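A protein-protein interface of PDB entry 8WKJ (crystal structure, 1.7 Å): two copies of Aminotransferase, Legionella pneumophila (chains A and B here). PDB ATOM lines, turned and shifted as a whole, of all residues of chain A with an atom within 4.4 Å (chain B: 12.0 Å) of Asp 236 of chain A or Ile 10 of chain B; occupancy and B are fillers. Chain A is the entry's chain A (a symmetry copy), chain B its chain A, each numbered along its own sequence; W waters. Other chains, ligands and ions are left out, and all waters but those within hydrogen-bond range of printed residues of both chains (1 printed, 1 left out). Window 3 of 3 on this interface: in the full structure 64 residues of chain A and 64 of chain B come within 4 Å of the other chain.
The side-chain amide nitrogen of Gln 17 of chain B is in hydrogen-bond range of the backbone carbonyl oxygen of Leu 12 of chain B (2.8 Å).
Among the printed residues, pairs that only touch across the chains: Pro 263 of chain A with Leu 12 of chain B (3.5 Å), Tyr 119 of chain A with Ala 11 of chain B (3.6 Å), Asp 236 of chain A with Ile 10 of chain B (3.6 Å), Tyr 119 of chain A with Ala 13 of chain B (3.6 Å), Pro 261 of chain A with Ile 10 of chain B (3.7 Å), Tyr 119 of chain A with Ile 10 of chain B (3.7 Å) and Leu 264 of chain A with Leu 12 of chain B (3.99 Å).
Of chain B, only Ile 10 (3.7 Å), Ala 11 (3.6 Å) and Ala 13 (3.6 Å) come within 4 Å of Tyr 119 of chain A. Glu 233 of chain A touches none of the printed residues of chain B. No residue of chain B comes within 4 Å of Leu 234 of chain A. Asp 236 of chain A touches just one residue of chain B: Ile 10. No residue of chain B comes within 4 Å of Arg 237 of chain A. Pro 261 of chain A touches one residue of chain B. Pro 263 of chain A touches one residue of chain B. Of the printed residues of chain B, Leu 264 of chain A touches Leu 12. Of chain A, only Tyr 119, Asp 236 and Pro 261 come within 4 Å of Ile 10 of chain B. Printed residues of chain A within 4 Å of Ala 11 of chain B: Tyr 119. Of the printed residues of chain A, Ala 13 of chain B touches Tyr 119. Lys 14 of chain B touches none of the printed residues of chain A.
Hydrophobic or aromatic side chains of chain B within 4 Å of the printed part of chain A: Ile 10, Leu 12 and Ala 13. Of the 10 printed residues of chain A, 5 touch a printed residue of chain B. Hydrophobic or aromatic side chains of chain A within 4 Å of the printed part of chain B: Tyr 119 and Pro 261.
No position is printed for both chains. Of the 7 pairs that touch across the chains among the printed residues, none has its exchanged pair printed and touching as well.
Water W1 lies within hydrogen-bond range of O of Tyr 119 of chain A (2.7 Å), O of Ala 11 of chain B (2.7 Å) and N of Ala 13 of chain B (3.5 Å).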
ATOM      1  N   TYR A 119     -11.565  19.767 -18.106  1.00  0.00           N
ATOM      2  CA  TYR A 119     -11.138  20.570 -16.960  1.00  0.00           C
ATOM      3  C   TYR A 119      -9.625  20.698 -16.806  1.00  0.00           C
ATOM      4  O   TYR A 119      -9.141  21.787 -16.470  1.00  0.00           O
ATOM      5  CB  TYR A 119     -11.746  19.969 -15.672  1.00  0.00           C
ATOM      6  CG  TYR A 119     -11.303  20.664 -14.402  1.00  0.00           C
ATOM      7  CD1 TYR A 119     -11.820  21.905 -14.047  1.00  0.00           C
ATOM      8  CD2 TYR A 119     -10.361  20.071 -13.558  1.00  0.00           C
ATOM      9  CE1 TYR A 119     -11.419  22.538 -12.883  1.00  0.00           C
ATOM     10  CE2 TYR A 119      -9.945  20.701 -12.401  1.00  0.00           C
ATOM     11  CZ  TYR A 119     -10.479  21.932 -12.070  1.00  0.00           C
ATOM     12  OH  TYR A 119     -10.069  22.561 -10.917  1.00  0.00           O
ATOM     13  N   GLU A 233     -20.758  22.875   2.024  1.00  0.00           N
ATOM     14  CA  GLU A 233     -20.169  24.086   1.472  1.00  0.00           C
ATOM     15  C   GLU A 233     -19.249  23.827   0.283  1.00  0.00           C
ATOM     16  O   GLU A 233     -18.868  24.788  -0.389  1.00  0.00           O
ATOM     17  CB  GLU A 233     -19.415  24.832   2.581  1.00  0.00           C
ATOM     18  CG  GLU A 233     -18.274  24.035   3.205  1.00  0.00           C
ATOM     19  CD  GLU A 233     -18.672  23.264   4.467  1.00  0.00           C
ATOM     20  OE1 GLU A 233     -19.848  22.859   4.606  1.00  0.00           O
ATOM     21  OE2 GLU A 233     -17.790  23.057   5.327  1.00  0.00           O
ATOM     22  N   LEU A 234     -18.887  22.573  -0.006  1.00  0.00           N
ATOM     23  CA  LEU A 234     -18.065  22.253  -1.173  1.00  0.00           C
ATOM     24  C   LEU A 234     -18.891  21.994  -2.428  1.00  0.00           C
ATOM     25  O   LEU A 234     -18.320  21.690  -3.483  1.00  0.00           O
ATOM     26  CB  LEU A 234     -17.175  21.039  -0.872  1.00  0.00           C
ATOM     27  CG  LEU A 234     -16.115  21.301   0.209  1.00  0.00           C
ATOM     28  CD1 LEU A 234     -15.429  20.009   0.640  1.00  0.00           C
ATOM     29  CD2 LEU A 234     -15.095  22.310  -0.293  1.00  0.00           C
ATOM     30  N   TYR A 235     -20.216  22.145  -2.341  1.00  0.00           N
ATOM     31  CA  TYR A 235     -21.105  21.862  -3.469  1.00  0.00           C
ATOM     32  C   TYR A 235     -20.668  22.554  -4.759  1.00  0.00           C
ATOM     33  O   TYR A 235     -20.701  21.949  -5.836  1.00  0.00           O
ATOM     34  CB  TYR A 235     -22.526  22.283  -3.091  1.00  0.00           C
ATOM     35  CG  TYR A 235     -23.563  22.178  -4.192  1.00  0.00           C
ATOM     36  CD1 TYR A 235     -23.785  23.236  -5.074  1.00  0.00           C
ATOM     37  CD2 TYR A 235     -24.371  21.050  -4.302  1.00  0.00           C
ATOM     38  CE1 TYR A 235     -24.745  23.152  -6.060  1.00  0.00           C
ATOM     39  CE2 TYR A 235     -25.341  20.963  -5.283  1.00  0.00           C
ATOM     40  CZ  TYR A 235     -25.521  22.015  -6.160  1.00  0.00           C
ATOM     41  OH  TYR A 235     -26.487  21.937  -7.140  1.00  0.00           O
ATOM     42  N   ASP A 236     -20.283  23.828  -4.686  1.00  0.00           N
ATOM     43  CA  ASP A 236     -20.004  24.563  -5.911  1.00  0.00           C
ATOM     44  C   ASP A 236     -18.663  24.200  -6.545  1.00  0.00           C
ATOM     45  O   ASP A 236     -18.338  24.732  -7.614  1.00  0.00           O
ATOM     46  CB  ASP A 236     -20.070  26.071  -5.650  1.00  0.00           C
ATOM     47  CG  ASP A 236     -19.033  26.540  -4.646  1.00  0.00           C
ATOM     48  OD1 ASP A 236     -18.313  25.690  -4.075  1.00  0.00           O
ATOM     49  OD2 ASP A 236     -18.950  27.766  -4.416  1.00  0.00           O
ATOM     50  N   ARG A 237     -17.884  23.305  -5.933  1.00  0.00           N
ATOM     51  CA  ARG A 237     -16.626  22.867  -6.528  1.00  0.00           C
ATOM     52  C   ARG A 237     -16.502  21.348  -6.487  1.00  0.00           C
ATOM     53  O   ARG A 237     -15.395  20.813  -6.419  1.00  0.00           O
ATOM     54  CB  ARG A 237     -15.430  23.529  -5.836  1.00  0.00           C
ATOM     55  CG  ARG A 237     -15.624  23.772  -4.349  1.00  0.00           C
ATOM     56  CD  ARG A 237     -14.429  24.501  -3.728  1.00  0.00           C
ATOM     57  NE  ARG A 237     -13.251  23.647  -3.749  1.00  0.00           N
ATOM     58  CZ  ARG A 237     -12.320  23.605  -2.804  1.00  0.00           C
ATOM     59  NH1 ARG A 237     -11.302  22.767  -2.953  1.00  0.00           N
ATOM     60  NH2 ARG A 237     -12.394  24.391  -1.723  1.00  0.00           N
ATOM     61  N   THR A 238     -17.627  20.637  -6.552  1.00  0.00           N
ATOM     62  CA  THR A 238     -17.625  19.181  -6.528  1.00  0.00           C
ATOM     63  C   THR A 238     -18.431  18.658  -7.704  1.00  0.00           C
ATOM     64  O   THR A 238     -19.502  19.183  -8.010  1.00  0.00           O
ATOM     65  CB  THR A 238     -18.213  18.642  -5.223  1.00  0.00           C
ATOM     66  OG1 THR A 238     -17.433  19.117  -4.126  1.00  0.00           O
ATOM     67  CG2 THR A 238     -18.217  17.109  -5.215  1.00  0.00           C
ATOM     68  N   PRO A 261     -21.218  21.527 -11.302  1.00  0.00           N
ATOM     69  CA  PRO A 261     -21.387  22.919 -11.745  1.00  0.00           C
ATOM     70  C   PRO A 261     -21.733  23.004 -13.225  1.00  0.00           C
ATOM     71  O   PRO A 261     -21.106  22.355 -14.063  1.00  0.00           O
ATOM     72  CB  PRO A 261     -20.023  23.549 -11.444  1.00  0.00           C
ATOM     73  CG  PRO A 261     -19.457  22.713 -10.334  1.00  0.00           C
ATOM     74  CD  PRO A 261     -19.928  21.305 -10.627  1.00  0.00           C
ATOM     75  N   PRO A 263     -21.265  25.133 -15.770  1.00  0.00           N
ATOM     76  CA  PRO A 263     -20.259  25.370 -16.826  1.00  0.00           C
ATOM     77  C   PRO A 263     -19.377  24.162 -17.090  1.00  0.00           C
ATOM     78  O   PRO A 263     -19.036  23.875 -18.249  1.00  0.00           O
ATOM     79  CB  PRO A 263     -19.453  26.561 -16.279  1.00  0.00           C
ATOM     80  CG  PRO A 263     -20.397  27.251 -15.338  1.00  0.00           C
ATOM     81  CD  PRO A 263     -21.148  26.126 -14.686  1.00  0.00           C
ATOM     82  N   LEU A 264     -19.021  23.430 -16.037  1.00  0.00           N
ATOM     83  CA  LEU A 264     -18.192  22.243 -16.195  1.00  0.00           C
ATOM     84  C   LEU A 264     -18.962  21.125 -16.883  1.00  0.00           C
ATOM     85  O   LEU A 264     -18.437  20.454 -17.780  1.00  0.00           O
ATOM     86  CB  LEU A 264     -17.688  21.788 -14.827  1.00  0.00           C
ATOM     87  CG  LEU A 264     -16.955  20.447 -14.826  1.00  0.00           C
ATOM     88  CD1 LEU A 264     -15.651  20.595 -15.573  1.00  0.00           C
ATOM     89  CD2 LEU A 264     -16.731  19.964 -13.389  1.00  0.00           C
ATOM     90  N   MET B   8     -16.583  31.398  -7.105  1.00  0.00           N
ATOM     91  CA  MET B   8     -15.946  31.407  -8.420  1.00  0.00           C
ATOM     92  C   MET B   8     -16.518  30.331  -9.328  1.00  0.00           C
ATOM     93  O   MET B   8     -16.754  29.203  -8.900  1.00  0.00           O
ATOM     94  CB  MET B   8     -14.436  31.209  -8.296  1.00  0.00           C
ATOM     95  CG  MET B   8     -13.825  31.851  -7.072  1.00  0.00           C
ATOM     96  SD  MET B   8     -12.070  31.467  -6.949  1.00  0.00           S
ATOM     97  CE  MET B   8     -11.573  32.606  -5.677  1.00  0.00           C
ATOM     98  N   ASP B   9     -16.739  30.698 -10.585  1.00  0.00           N
ATOM     99  CA  ASP B   9     -17.103  29.724 -11.596  1.00  0.00           C
ATOM    100  C   ASP B   9     -15.946  28.763 -11.839  1.00  0.00           C
ATOM    101  O   ASP B   9     -14.770  29.133 -11.772  1.00  0.00           O
ATOM    102  CB  ASP B   9     -17.483  30.420 -12.903  1.00  0.00           C
ATOM    103  CG  ASP B   9     -18.839  31.101 -12.828  1.00  0.00           C
ATOM    104  OD1 ASP B   9     -19.315  31.350 -11.700  1.00  0.00           O
ATOM    105  OD2 ASP B   9     -19.427  31.381 -13.897  1.00  0.00           O
ATOM    106  N   ILE B  10     -16.293  27.507 -12.100  1.00  0.00           N
ATOM    107  CA  ILE B  10     -15.283  26.532 -12.485  1.00  0.00           C
ATOM    108  C   ILE B  10     -14.763  26.893 -13.869  1.00  0.00           C
ATOM    109  O   ILE B  10     -15.540  27.075 -14.814  1.00  0.00           O
ATOM    110  CB  ILE B  10     -15.867  25.112 -12.449  1.00  0.00           C
ATOM    111  CG1 ILE B  10     -16.488  24.814 -11.079  1.00  0.00           C
ATOM    112  CG2 ILE B  10     -14.814  24.071 -12.837  1.00  0.00           C
ATOM    113  CD1 ILE B  10     -15.596  25.131  -9.870  1.00  0.00           C
ATOM    114  N   ALA B  11     -13.444  27.027 -13.988  1.00  0.00           N
ATOM    115  CA  ALA B  11     -12.824  27.305 -15.275  1.00  0.00           C
ATOM    116  C   ALA B  11     -12.810  26.057 -16.149  1.00  0.00           C
ATOM    117  O   ALA B  11     -12.795  24.922 -15.659  1.00  0.00           O
ATOM    118  CB  ALA B  11     -11.399  27.819 -15.080  1.00  0.00           C
ATOM    119  N   LEU B  12     -12.794  26.275 -17.463  1.00  0.00           N
ATOM    120  CA  LEU B  12     -12.775  25.186 -18.428  1.00  0.00           C
ATOM    121  C   LEU B  12     -11.378  25.018 -19.019  1.00  0.00           C
ATOM    122  O   LEU B  12     -10.639  25.990 -19.197  1.00  0.00           O
ATOM    123  CB  LEU B  12     -13.788  25.440 -19.542  1.00  0.00           C
ATOM    124  CG  LEU B  12     -15.184  25.805 -19.015  1.00  0.00           C
ATOM    125  CD1 LEU B  12     -16.148  26.027 -20.167  1.00  0.00           C
ATOM    126  CD2 LEU B  12     -15.686  24.724 -18.071  1.00  0.00           C
ATOM    127  N   ALA B  13     -11.019  23.765 -19.306  1.00  0.00           N
ATOM    128  CA  ALA B  13      -9.730  23.467 -19.915  1.00  0.00           C
ATOM    129  C   ALA B  13      -9.510  24.303 -21.171  1.00  0.00           C
ATOM    130  O   ALA B  13     -10.438  24.580 -21.937  1.00  0.00           O
ATOM    131  CB  ALA B  13      -9.640  21.977 -20.271  1.00  0.00           C
ATOM    132  N   LYS B  14      -8.253  24.685 -21.394  1.00  0.00           N
ATOM    133  CA  LYS B  14      -7.918  25.434 -22.600  1.00  0.00           C
ATOM    134  C   LYS B  14      -8.348  24.692 -23.867  1.00  0.00           C
ATOM    135  O   LYS B  14      -8.794  25.324 -24.833  1.00  0.00           O
ATOM    136  CB  LYS B  14      -6.419  25.730 -22.625  1.00  0.00           C
ATOM    137  CG  LYS B  14      -6.008  26.837 -21.659  1.00  0.00           C
ATOM    138  CD  LYS B  14      -4.494  26.932 -21.527  1.00  0.00           C
ATOM    139  CE  LYS B  14      -4.089  27.495 -20.167  1.00  0.00           C
ATOM    140  NZ  LYS B  14      -3.044  26.657 -19.508  1.00  0.00           N
ATOM    141  N   VAL B  16     -10.927  22.817 -24.454  1.00  0.00           N
ATOM    142  CA  VAL B  16     -12.355  22.862 -24.763  1.00  0.00           C
ATOM    143  C   VAL B  16     -12.784  24.286 -25.119  1.00  0.00           C
ATOM    144  O   VAL B  16     -13.802  24.474 -25.796  1.00  0.00           O
ATOM    145  CB  VAL B  16     -13.152  22.219 -23.607  1.00  0.00           C
ATOM    146  CG1 VAL B  16     -13.403  23.192 -22.483  1.00  0.00           C
ATOM    147  CG2 VAL B  16     -14.470  21.622 -24.115  1.00  0.00           C
ATOM    148  N   GLN B  17     -12.001  25.296 -24.748  1.00  0.00           N
ATOM    149  CA  GLN B  17     -12.274  26.650 -25.217  1.00  0.00           C
ATOM    150  C   GLN B  17     -12.000  26.814 -26.707  1.00  0.00           C
ATOM    151  O   GLN B  17     -12.449  27.802 -27.302  1.00  0.00           O
ATOM    152  CB  GLN B  17     -11.444  27.654 -24.413  1.00  0.00           C
ATOM    153  CG  GLN B  17     -11.721  27.626 -22.908  1.00  0.00           C
ATOM    154  CD  GLN B  17     -10.801  28.554 -22.131  1.00  0.00           C
ATOM    155  OE1 GLN B  17     -10.495  29.653 -22.587  1.00  0.00           O
ATOM    156  NE2 GLN B  17     -10.351  28.113 -20.959  1.00  0.00           N
HETATM  157  O   HOH W   1     -10.232  24.164 -15.965  1.00  0.00           O
